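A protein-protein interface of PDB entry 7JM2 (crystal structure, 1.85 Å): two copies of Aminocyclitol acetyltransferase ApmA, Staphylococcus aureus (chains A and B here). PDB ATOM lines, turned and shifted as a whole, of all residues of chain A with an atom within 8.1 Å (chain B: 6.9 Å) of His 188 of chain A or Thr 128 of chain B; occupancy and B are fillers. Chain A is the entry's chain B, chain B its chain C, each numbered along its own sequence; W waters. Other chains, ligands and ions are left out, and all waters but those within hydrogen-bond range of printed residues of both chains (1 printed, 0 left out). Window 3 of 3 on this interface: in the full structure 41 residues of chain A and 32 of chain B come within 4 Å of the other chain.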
ATOM      1  N   ASN A 126      -9.645   8.435 -20.648  1.00  0.00           N
ATOM      2  CA  ASN A 126      -8.254   8.342 -21.077  1.00  0.00           C
ATOM      3  C   ASN A 126      -7.351   9.114 -20.128  1.00  0.00           C
ATOM      4  O   ASN A 126      -7.702  10.196 -19.646  1.00  0.00           O
ATOM      5  CB  ASN A 126      -8.094   8.883 -22.496  1.00  0.00           C
ATOM      6  CG  ASN A 126      -6.767   8.499 -23.107  1.00  0.00           C
ATOM      7  OD1 ASN A 126      -5.775   9.206 -22.942  1.00  0.00           O
ATOM      8  ND2 ASN A 126      -6.735   7.362 -23.799  1.00  0.00           N
ATOM      9  N   GLY A 127      -6.175   8.548 -19.867  1.00  0.00           N
ATOM     10  CA  GLY A 127      -5.251   9.159 -18.926  1.00  0.00           C
ATOM     11  C   GLY A 127      -4.710  10.519 -19.333  1.00  0.00           C
ATOM     12  O   GLY A 127      -4.206  11.250 -18.474  1.00  0.00           O
ATOM     13  N   THR A 128      -4.763  10.867 -20.619  1.00  0.00           N
ATOM     14  CA  THR A 128      -4.232  12.153 -21.056  1.00  0.00           C
ATOM     15  C   THR A 128      -5.282  13.256 -21.044  1.00  0.00           C
ATOM     16  O   THR A 128      -4.962  14.400 -21.384  1.00  0.00           O
ATOM     17  CB  THR A 128      -3.618  12.056 -22.456  1.00  0.00           C
ATOM     18  OG1 THR A 128      -4.619  11.653 -23.404  1.00  0.00           O
ATOM     19  CG2 THR A 128      -2.473  11.051 -22.469  1.00  0.00           C
ATOM     20  N   ALA A 129      -6.513  12.951 -20.647  1.00  0.00           N
ATOM     21  CA  ALA A 129      -7.536  13.989 -20.563  1.00  0.00           C
ATOM     22  C   ALA A 129      -7.226  14.969 -19.435  1.00  0.00           C
ATOM     23  O   ALA A 129      -6.632  14.607 -18.420  1.00  0.00           O
ATOM     24  CB  ALA A 129      -8.909  13.362 -20.345  1.00  0.00           C
ATOM     25  N   GLU A 130      -7.642  16.224 -19.618  1.00  0.00           N
ATOM     26  CA  GLU A 130      -7.320  17.292 -18.678  1.00  0.00           C
ATOM     27  C   GLU A 130      -8.576  18.073 -18.332  1.00  0.00           C
ATOM     28  O   GLU A 130      -9.448  18.274 -19.180  1.00  0.00           O
ATOM     29  CB  GLU A 130      -6.263  18.255 -19.245  1.00  0.00           C
ATOM     30  CG  GLU A 130      -4.889  17.631 -19.435  1.00  0.00           C
ATOM     31  CD  GLU A 130      -4.183  17.297 -18.125  1.00  0.00           C
ATOM     32  OE1 GLU A 130      -4.505  17.909 -17.089  1.00  0.00           O
ATOM     33  OE2 GLU A 130      -3.291  16.421 -18.139  1.00  0.00           O
ATOM     34  N   ILE A 185     -14.266   9.161 -22.463  1.00  0.00           N
ATOM     35  CA  ILE A 185     -13.520  10.381 -22.762  1.00  0.00           C
ATOM     36  C   ILE A 185     -12.202   9.981 -23.414  1.00  0.00           C
ATOM     37  O   ILE A 185     -11.419   9.223 -22.827  1.00  0.00           O
ATOM     38  CB  ILE A 185     -13.283  11.213 -21.493  1.00  0.00           C
ATOM     39  CG1 ILE A 185     -14.632  11.577 -20.854  1.00  0.00           C
ATOM     40  CG2 ILE A 185     -12.510  12.463 -21.819  1.00  0.00           C
ATOM     41  CD1 ILE A 185     -14.527  12.509 -19.662  1.00  0.00           C
ATOM     42  N   GLY A 186     -11.964  10.470 -24.634  1.00  0.00           N
ATOM     43  CA  GLY A 186     -10.839  10.027 -25.427  1.00  0.00           C
ATOM     44  C   GLY A 186      -9.560  10.775 -25.108  1.00  0.00           C
ATOM     45  O   GLY A 186      -9.528  11.704 -24.306  1.00  0.00           O
ATOM     46  N   ALA A 187      -8.482  10.343 -25.765  1.00  0.00           N
ATOM     47  CA  ALA A 187      -7.165  10.936 -25.551  1.00  0.00           C
ATOM     48  C   ALA A 187      -7.154  12.441 -25.815  1.00  0.00           C
ATOM     49  O   ALA A 187      -7.776  12.928 -26.761  1.00  0.00           O
ATOM     50  CB  ALA A 187      -6.142  10.245 -26.453  1.00  0.00           C
ATOM     51  N   HIS A 188      -6.417  13.175 -24.970  1.00  0.00           N
ATOM     52  CA  HIS A 188      -6.160  14.613 -25.099  1.00  0.00           C
ATOM     53  C   HIS A 188      -7.426  15.463 -25.017  1.00  0.00           C
ATOM     54  O   HIS A 188      -7.429  16.607 -25.468  1.00  0.00           O
ATOM     55  CB  HIS A 188      -5.418  14.945 -26.396  1.00  0.00           C
ATOM     56  CG  HIS A 188      -4.119  14.224 -26.543  1.00  0.00           C
ATOM     57  ND1 HIS A 188      -3.749  13.591 -27.710  1.00  0.00           N
ATOM     58  CD2 HIS A 188      -3.100  14.036 -25.672  1.00  0.00           C
ATOM     59  CE1 HIS A 188      -2.560  13.040 -27.549  1.00  0.00           C
ATOM     60  NE2 HIS A 188      -2.145  13.295 -26.321  1.00  0.00           N
ATOM     61  N   ALA A 189      -8.515  14.921 -24.498  1.00  0.00           N
ATOM     62  CA  ALA A 189      -9.708  15.726 -24.310  1.00  0.00           C
ATOM     63  C   ALA A 189      -9.492  16.737 -23.192  1.00  0.00           C
ATOM     64  O   ALA A 189      -8.642  16.570 -22.315  1.00  0.00           O
ATOM     65  CB  ALA A 189     -10.910  14.840 -23.988  1.00  0.00           C
ATOM     66  N   PHE A 190     -10.297  17.785 -23.217  1.00  0.00           N
ATOM     67  CA  PHE A 190     -10.236  18.821 -22.203  1.00  0.00           C
ATOM     68  C   PHE A 190     -11.653  19.209 -21.819  1.00  0.00           C
ATOM     69  O   PHE A 190     -12.512  19.345 -22.693  1.00  0.00           O
ATOM     70  CB  PHE A 190      -9.480  20.041 -22.724  1.00  0.00           C
ATOM     71  CG  PHE A 190      -9.640  21.249 -21.865  1.00  0.00           C
ATOM     72  CD1 PHE A 190      -8.888  21.385 -20.716  1.00  0.00           C
ATOM     73  CD2 PHE A 190     -10.558  22.244 -22.192  1.00  0.00           C
ATOM     74  CE1 PHE A 190      -9.035  22.504 -19.914  1.00  0.00           C
ATOM     75  CE2 PHE A 190     -10.712  23.364 -21.396  1.00  0.00           C
ATOM     76  CZ  PHE A 190      -9.954  23.493 -20.255  1.00  0.00           C
ATOM     77  N   ILE A 191     -11.907  19.373 -20.521  1.00  0.00           N
ATOM     78  CA  ILE A 191     -13.186  19.892 -20.038  1.00  0.00           C
ATOM     79  C   ILE A 191     -12.913  21.130 -19.195  1.00  0.00           C
ATOM     80  O   ILE A 191     -12.062  21.098 -18.298  1.00  0.00           O
ATOM     81  CB  ILE A 191     -13.975  18.851 -19.222  1.00  0.00           C
ATOM     82  CG1 ILE A 191     -14.053  17.519 -19.971  1.00  0.00           C
ATOM     83  CG2 ILE A 191     -15.375  19.396 -18.888  1.00  0.00           C
ATOM     84  CD1 ILE A 191     -14.827  16.445 -19.226  1.00  0.00           C
ATOM     85  N   ILE A 205     -16.972  11.645 -25.376  1.00  0.00           N
ATOM     86  CA  ILE A 205     -16.165  12.810 -25.698  1.00  0.00           C
ATOM     87  C   ILE A 205     -15.002  12.310 -26.535  1.00  0.00           C
ATOM     88  O   ILE A 205     -14.148  11.564 -26.041  1.00  0.00           O
ATOM     89  CB  ILE A 205     -15.686  13.534 -24.433  1.00  0.00           C
ATOM     90  CG1 ILE A 205     -16.899  14.056 -23.646  1.00  0.00           C
ATOM     91  CG2 ILE A 205     -14.739  14.669 -24.786  1.00  0.00           C
ATOM     92  CD1 ILE A 205     -16.546  14.757 -22.348  1.00  0.00           C
ATOM     93  N   GLY A 206     -14.973  12.713 -27.801  1.00  0.00           N
ATOM     94  CA  GLY A 206     -13.984  12.190 -28.714  1.00  0.00           C
ATOM     95  C   GLY A 206     -12.587  12.663 -28.380  1.00  0.00           C
ATOM     96  O   GLY A 206     -12.380  13.663 -27.686  1.00  0.00           O
ATOM     97  N   SER A 207     -11.609  11.919 -28.896  1.00  0.00           N
ATOM     98  CA  SER A 207     -10.213  12.288 -28.726  1.00  0.00           C
ATOM     99  C   SER A 207      -9.997  13.713 -29.225  1.00  0.00           C
ATOM    100  O   SER A 207     -10.501  14.098 -30.283  1.00  0.00           O
ATOM    101  CB  SER A 207      -9.328  11.305 -29.511  1.00  0.00           C
ATOM    102  OG  SER A 207      -9.199  10.066 -28.814  1.00  0.00           O
ATOM    103  N   GLY A 208      -9.267  14.514 -28.446  1.00  0.00           N
ATOM    104  CA  GLY A 208      -8.978  15.869 -28.866  1.00  0.00           C
ATOM    105  C   GLY A 208     -10.107  16.873 -28.699  1.00  0.00           C
ATOM    106  O   GLY A 208      -9.920  18.042 -29.049  1.00  0.00           O
ATOM    107  N   ALA A 209     -11.266  16.460 -28.184  1.00  0.00           N
ATOM    108  CA  ALA A 209     -12.390  17.372 -28.007  1.00  0.00           C
ATOM    109  C   ALA A 209     -12.130  18.353 -26.872  1.00  0.00           C
ATOM    110  O   ALA A 209     -11.576  17.994 -25.827  1.00  0.00           O
ATOM    111  CB  ALA A 209     -13.675  16.592 -27.726  1.00  0.00           C
ATOM    112  N   VAL A 210     -12.548  19.599 -27.074  1.00  0.00           N
ATOM    113  CA  VAL A 210     -12.377  20.659 -26.086  1.00  0.00           C
ATOM    114  C   VAL A 210     -13.768  21.086 -25.630  1.00  0.00           C
ATOM    115  O   VAL A 210     -14.455  21.860 -26.309  1.00  0.00           O
ATOM    116  CB  VAL A 210     -11.569  21.829 -26.647  1.00  0.00           C
ATOM    117  CG1 VAL A 210     -11.621  23.040 -25.713  1.00  0.00           C
ATOM    118  CG2 VAL A 210     -10.117  21.355 -26.881  1.00  0.00           C
ATOM    119  N   VAL A 211     -14.185  20.586 -24.474  1.00  0.00           N
ATOM    120  CA  VAL A 211     -15.566  20.705 -24.015  1.00  0.00           C
ATOM    121  C   VAL A 211     -15.697  21.966 -23.162  1.00  0.00           C
ATOM    122  O   VAL A 211     -15.141  22.043 -22.060  1.00  0.00           O
ATOM    123  CB  VAL A 211     -15.993  19.461 -23.228  1.00  0.00           C
ATOM    124  CG1 VAL A 211     -17.441  19.563 -22.835  1.00  0.00           C
ATOM    125  CG2 VAL A 211     -15.706  18.169 -24.038  1.00  0.00           C
ATOM    126  N   VAL A 224     -12.775  21.078 -31.651  1.00  0.00           N
ATOM    127  CA  VAL A 224     -12.253  22.186 -30.863  1.00  0.00           C
ATOM    128  C   VAL A 224     -12.913  23.473 -31.356  1.00  0.00           C
ATOM    129  O   VAL A 224     -12.514  24.033 -32.377  1.00  0.00           O
ATOM    130  CB  VAL A 224     -10.720  22.286 -30.978  1.00  0.00           C
ATOM    131  CG1 VAL A 224     -10.172  23.326 -29.990  1.00  0.00           C
ATOM    132  CG2 VAL A 224     -10.061  20.935 -30.781  1.00  0.00           C
ATOM    133  N   GLY B 104       7.067   7.466 -28.787  1.00  0.00           N
ATOM    134  CA  GLY B 104       6.930   7.605 -27.353  1.00  0.00           C
ATOM    135  C   GLY B 104       6.084   6.515 -26.724  1.00  0.00           C
ATOM    136  O   GLY B 104       5.689   5.535 -27.359  1.00  0.00           O
ATOM    137  N   ASP B 105       5.761   6.736 -25.444  1.00  0.00           N
ATOM    138  CA  ASP B 105       5.176   5.679 -24.627  1.00  0.00           C
ATOM    139  C   ASP B 105       3.785   5.284 -25.103  1.00  0.00           C
ATOM    140  O   ASP B 105       3.381   4.132 -24.918  1.00  0.00           O
ATOM    141  CB  ASP B 105       5.142   6.102 -23.158  1.00  0.00           C
ATOM    142  CG  ASP B 105       6.538   6.219 -22.549  1.00  0.00           C
ATOM    143  OD1 ASP B 105       7.427   5.418 -22.920  1.00  0.00           O
ATOM    144  OD2 ASP B 105       6.744   7.106 -21.690  1.00  0.00           O
ATOM    145  N   GLY B 106       3.037   6.211 -25.708  1.00  0.00           N
ATOM    146  CA  GLY B 106       1.736   5.849 -26.257  1.00  0.00           C
ATOM    147  C   GLY B 106       1.843   4.847 -27.390  1.00  0.00           C
ATOM    148  O   GLY B 106       1.063   3.890 -27.462  1.00  0.00           O
ATOM    149  N   ILE B 125       8.086  10.067 -34.653  1.00  0.00           N
ATOM    150  CA  ILE B 125       6.793  10.180 -34.001  1.00  0.00           C
ATOM    151  C   ILE B 125       6.976  10.893 -32.677  1.00  0.00           C
ATOM    152  O   ILE B 125       7.669  10.396 -31.777  1.00  0.00           O
ATOM    153  CB  ILE B 125       6.116   8.821 -33.797  1.00  0.00           C
ATOM    154  CG1 ILE B 125       6.024   8.077 -35.134  1.00  0.00           C
ATOM    155  CG2 ILE B 125       4.747   9.033 -33.184  1.00  0.00           C
ATOM    156  CD1 ILE B 125       5.331   6.744 -35.043  1.00  0.00           C
ATOM    157  N   ASN B 126       6.356  12.056 -32.564  1.00  0.00           N
ATOM    158  CA  ASN B 126       6.425  12.828 -31.339  1.00  0.00           C
ATOM    159  C   ASN B 126       5.991  11.996 -30.133  1.00  0.00           C
ATOM    160  O   ASN B 126       5.077  11.167 -30.213  1.00  0.00           O
ATOM    161  CB  ASN B 126       5.549  14.069 -31.481  1.00  0.00           C
ATOM    162  CG  ASN B 126       5.696  14.997 -30.325  1.00  0.00           C
ATOM    163  OD1 ASN B 126       5.088  14.789 -29.270  1.00  0.00           O
ATOM    164  ND2 ASN B 126       6.501  16.039 -30.504  1.00  0.00           N
ATOM    165  N   GLY B 127       6.651  12.246 -29.002  1.00  0.00           N
ATOM    166  CA  GLY B 127       6.440  11.465 -27.798  1.00  0.00           C
ATOM    167  C   GLY B 127       5.053  11.569 -27.191  1.00  0.00           C
ATOM    168  O   GLY B 127       4.675  10.695 -26.406  1.00  0.00           O
ATOM    169  N   THR B 128       4.287  12.613 -27.519  1.00  0.00           N
ATOM    170  CA  THR B 128       2.938  12.755 -26.992  1.00  0.00           C
ATOM    171  C   THR B 128       1.865  12.215 -27.934  1.00  0.00           C
ATOM    172  O   THR B 128       0.675  12.365 -27.643  1.00  0.00           O
ATOM    173  CB  THR B 128       2.630  14.226 -26.649  1.00  0.00           C
ATOM    174  OG1 THR B 128       2.671  15.032 -27.833  1.00  0.00           O
ATOM    175  CG2 THR B 128       3.631  14.762 -25.651  1.00  0.00           C
ATOM    176  N   ALA B 129       2.249  11.594 -29.051  1.00  0.00           N
ATOM    177  CA  ALA B 129       1.258  10.973 -29.922  1.00  0.00           C
ATOM    178  C   ALA B 129       0.619   9.769 -29.233  1.00  0.00           C
ATOM    179  O   ALA B 129       1.250   9.076 -28.433  1.00  0.00           O
ATOM    180  CB  ALA B 129       1.896  10.545 -31.243  1.00  0.00           C
ATOM    181  N   GLU B 130      -0.660   9.530 -29.536  1.00  0.00           N
ATOM    182  CA  GLU B 130      -1.414   8.461 -28.890  1.00  0.00           C
ATOM    183  C   GLU B 130      -2.101   7.617 -29.951  1.00  0.00           C
ATOM    184  O   GLU B 130      -2.468   8.113 -31.019  1.00  0.00           O
ATOM    185  CB  GLU B 130      -2.468   9.008 -27.884  1.00  0.00           C
ATOM    186  CG  GLU B 130      -1.889   9.830 -26.734  1.00  0.00           C
ATOM    187  CD  GLU B 130      -1.185   8.983 -25.677  1.00  0.00           C
ATOM    188  OE1 GLU B 130      -1.433   7.756 -25.624  1.00  0.00           O
ATOM    189  OE2 GLU B 130      -0.382   9.542 -24.890  1.00  0.00           O
ATOM    190  N   HIS B 132      -5.098   4.611 -29.808  1.00  0.00           N
ATOM    191  CA  HIS B 132      -6.064   3.807 -29.064  1.00  0.00           C
ATOM    192  C   HIS B 132      -7.171   3.367 -30.013  1.00  0.00           C
ATOM    193  O   HIS B 132      -7.459   4.049 -31.001  1.00  0.00           O
ATOM    194  CB  HIS B 132      -6.723   4.570 -27.898  1.00  0.00           C
ATOM    195  CG  HIS B 132      -5.767   5.251 -26.965  1.00  0.00           C
ATOM    196  ND1 HIS B 132      -4.878   4.562 -26.169  1.00  0.00           N
ATOM    197  CD2 HIS B 132      -5.606   6.561 -26.658  1.00  0.00           C
ATOM    198  CE1 HIS B 132      -4.188   5.421 -25.436  1.00  0.00           C
ATOM    199  NE2 HIS B 132      -4.613   6.638 -25.711  1.00  0.00           N
ATOM    200  N   GLY B 186       3.335  14.663 -35.376  1.00  0.00           N
ATOM    201  CA  GLY B 186       3.606  15.732 -34.439  1.00  0.00           C
ATOM    202  C   GLY B 186       2.895  15.554 -33.104  1.00  0.00           C
ATOM    203  O   GLY B 186       2.193  14.570 -32.865  1.00  0.00           O
ATOM    204  N   ALA B 187       3.102  16.540 -32.227  1.00  0.00           N
ATOM    205  CA  ALA B 187       2.624  16.489 -30.845  1.00  0.00           C
ATOM    206  C   ALA B 187       1.109  16.368 -30.759  1.00  0.00           C
ATOM    207  O   ALA B 187       0.377  16.972 -31.542  1.00  0.00           O
ATOM    208  CB  ALA B 187       3.067  17.754 -30.092  1.00  0.00           C
ATOM    209  N   HIS B 188       0.635  15.615 -29.761  1.00  0.00           N
ATOM    210  CA  HIS B 188      -0.784  15.482 -29.429  1.00  0.00           C
ATOM    211  C   HIS B 188      -1.597  14.891 -30.565  1.00  0.00           C
ATOM    212  O   HIS B 188      -2.832  14.992 -30.560  1.00  0.00           O
ATOM    213  CB  HIS B 188      -1.416  16.819 -29.013  1.00  0.00           C
ATOM    214  CG  HIS B 188      -0.675  17.534 -27.933  1.00  0.00           C
ATOM    215  ND1 HIS B 188      -0.348  16.938 -26.735  1.00  0.00           N
ATOM    216  CD2 HIS B 188      -0.195  18.800 -27.869  1.00  0.00           C
ATOM    217  CE1 HIS B 188       0.295  17.806 -25.975  1.00  0.00           C
ATOM    218  NE2 HIS B 188       0.406  18.941 -26.642  1.00  0.00           N
ATOM    219  N   ALA B 189      -0.940  14.292 -31.549  1.00  0.00           N
ATOM    220  CA  ALA B 189      -1.665  13.618 -32.606  1.00  0.00           C
ATOM    221  C   ALA B 189      -2.305  12.346 -32.059  1.00  0.00           C
ATOM    222  O   ALA B 189      -1.884  11.790 -31.041  1.00  0.00           O
ATOM    223  CB  ALA B 189      -0.735  13.297 -33.775  1.00  0.00           C
ATOM    224  N   PHE B 190      -3.341  11.882 -32.754  1.00  0.00           N
ATOM    225  CA  PHE B 190      -4.044  10.673 -32.359  1.00  0.00           C
ATOM    226  C   PHE B 190      -4.377   9.857 -33.601  1.00  0.00           C
ATOM    227  O   PHE B 190      -4.757  10.412 -34.633  1.00  0.00           O
ATOM    228  CB  PHE B 190      -5.325  11.007 -31.574  1.00  0.00           C
ATOM    229  CG  PHE B 190      -6.239   9.831 -31.383  1.00  0.00           C
ATOM    230  CD1 PHE B 190      -6.002   8.918 -30.373  1.00  0.00           C
ATOM    231  CD2 PHE B 190      -7.324   9.631 -32.224  1.00  0.00           C
ATOM    232  CE1 PHE B 190      -6.834   7.821 -30.205  1.00  0.00           C
ATOM    233  CE2 PHE B 190      -8.160   8.535 -32.064  1.00  0.00           C
ATOM    234  CZ  PHE B 190      -7.914   7.630 -31.052  1.00  0.00           C
ATOM    235  N   GLY B 208      -1.685  17.816 -33.117  1.00  0.00           N
ATOM    236  CA  GLY B 208      -3.099  17.917 -32.804  1.00  0.00           C
ATOM    237  C   GLY B 208      -4.028  17.190 -33.761  1.00  0.00           C
ATOM    238  O   GLY B 208      -5.239  17.161 -33.517  1.00  0.00           O
ATOM    239  N   ALA B 209      -3.513  16.612 -34.842  1.00  0.00           N
ATOM    240  CA  ALA B 209      -4.389  15.939 -35.797  1.00  0.00           C
ATOM    241  C   ALA B 209      -5.042  14.720 -35.164  1.00  0.00           C
ATOM    242  O   ALA B 209      -4.420  13.993 -34.385  1.00  0.00           O
ATOM    243  CB  ALA B 209      -3.612  15.529 -37.044  1.00  0.00           C
ATOM    244  N   VAL B 210      -6.303  14.484 -35.509  1.00  0.00           N
ATOM    245  CA  VAL B 210      -7.038  13.326 -35.013  1.00  0.00           C
ATOM    246  C   VAL B 210      -7.361  12.458 -36.223  1.00  0.00           C
ATOM    247  O   VAL B 210      -8.301  12.739 -36.976  1.00  0.00           O
ATOM    248  CB  VAL B 210      -8.294  13.734 -34.232  1.00  0.00           C
ATOM    249  CG1 VAL B 210      -9.101  12.509 -33.821  1.00  0.00           C
ATOM    250  CG2 VAL B 210      -7.892  14.526 -32.988  1.00  0.00           C
HETATM  251  O   HOH W   1       0.098  12.336 -24.891  1.00  0.00           O
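NE2 of His 188 of chain A is in hydrogen-bond range of O of Thr 128 of chain B (3.3 Å). The side-chain amide nitrogen (ND2) of Asn 126 of chain A lies within hydrogen-bond range of a ring nitrogen (NE2) of His 132 of chain B. ND1 of His 188 of chain A is in hydrogen-bond range of O of His 188 of chain B (3.3 Å).
OG1 of Thr 128 of chain A sits at hydrogen-bond distance from N of His 188 of chain A (2.8 Å). N of Phe 190 of chain B is in hydrogen-bond range of O of Ala 209 of chain B (2.9 Å). The side-chain hydroxyl of Thr 128 of chain B is in hydrogen-bond range of the backbone NH of His 188 of chain B. The backbone NH (N) of Ala 187 of chain A sits at hydrogen-bond distance from the side-chain hydroxyl (OG) of Ser 207 of chain A. OG1 of Thr 128 of chain B is in hydrogen-bond range of OD1 of Asn 126 of chain B (2.8 Å). The backbone carbonyl oxygen (O) of Ala 189 of chain B lies within hydrogen-bond range of the backbone NH (N) of Glu 130 of chain B (3.0 Å).
Among the printed residues, pairs that only touch across the chains: His 188 of chain A with Glu 130 of chain B (3.4 Å), Thr 128 of chain A with Glu 130 of chain B (3.5 Å), Ser 207 of chain A with Phe 190 of chain B (3.5 Å), Ala 187 of chain A with His 132 of chain B (3.7 Å), His 188 of chain A with Ala 189 of chain B (3.8 Å) and Ser 207 of chain A with Val 210 of chain B (3.8 Å).
Of chain A, only His 188 (3.3 Å) comes within 4 Å of Thr 128 of chain B. Ala 129 of chain B touches none of the printed residues of chain A. Of the printed residues of chain A, Val 210 of chain B touches Ser 207 (3.8 Å). Printed residues of chain B within 4 Å of Asn 126 of chain A: His 132. Of the printed residues of chain A, Glu 130 of chain B touches Thr 128 (3.5 Å) and His 188 (3.4 Å). Of the printed residues of chain B, Thr 128 of chain A touches Glu 130 (3.5 Å). Printed residues of chain B within 4 Å of Ala 187 of chain A: His 132. Ile 205 of chain A touches none of the printed residues of chain B. Gly 208 of chain B touches none of the printed residues of chain A. The nearest residue of chain B that does not touch His 188 of chain A is Ala 129 of chain B (4.9 Å). The nearest residue of chain A that does not touch Thr 128 of chain B is Thr 128 of chain A (6.2 Å). The nearest printed residue of chain A that does not touch Glu 130 of chain B is Ala 187 of chain A (4.1 Å).
Hydrophobic or aromatic side chains of chain B that line the printed part of chain A: His 132, Phe 190 and Val 210. Printed residues of chain A that touch a printed residue of chain B: Asn 126, Thr 128, Ala 187, His 188 and Ser 207. Among the printed residues, 9 pairs touch across the chains. Among the printed residues, no Asp or Glu carboxylate lies within 4 Å of a Lys or Arg side-chain nitrogen of the other chain.
Thr 128 of chain A touches Glu 130 of chain B, but with the chains exchanged Glu 130 of chain A does not touch Thr 128 of chain B (10.3 Å). His 188 of chain A touches Thr 128 of chain B, but with the chains exchanged Thr 128 of chain A does not touch His 188 of chain B (7.3 Å). His 188 of chain A touches Glu 130 of chain B, but with the chains exchanged Glu 130 of chain A does not touch His 188 of chain B (8.3 Å). His 188 of chain A touches Ala 189 of chain B, but with the chains exchanged Ala 189 of chain A does not touch His 188 of chain B (8.3 Å). Positions printed for both chains: 126, 127, 128, 129, 130, 186, 187, 188, 189, 190, 208, 209 and 210. Of the 9 pairs that touch across the chains among the printed residues, 1 has its exchanged pair printed and touching as well.
Water W1 lies within hydrogen-bond range of O of Thr 128 of chain B (2.8 Å), NE2 of His 188 of chain A (2.8 Å) and OE2 of Glu 130 of chain B (2.8 Å).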
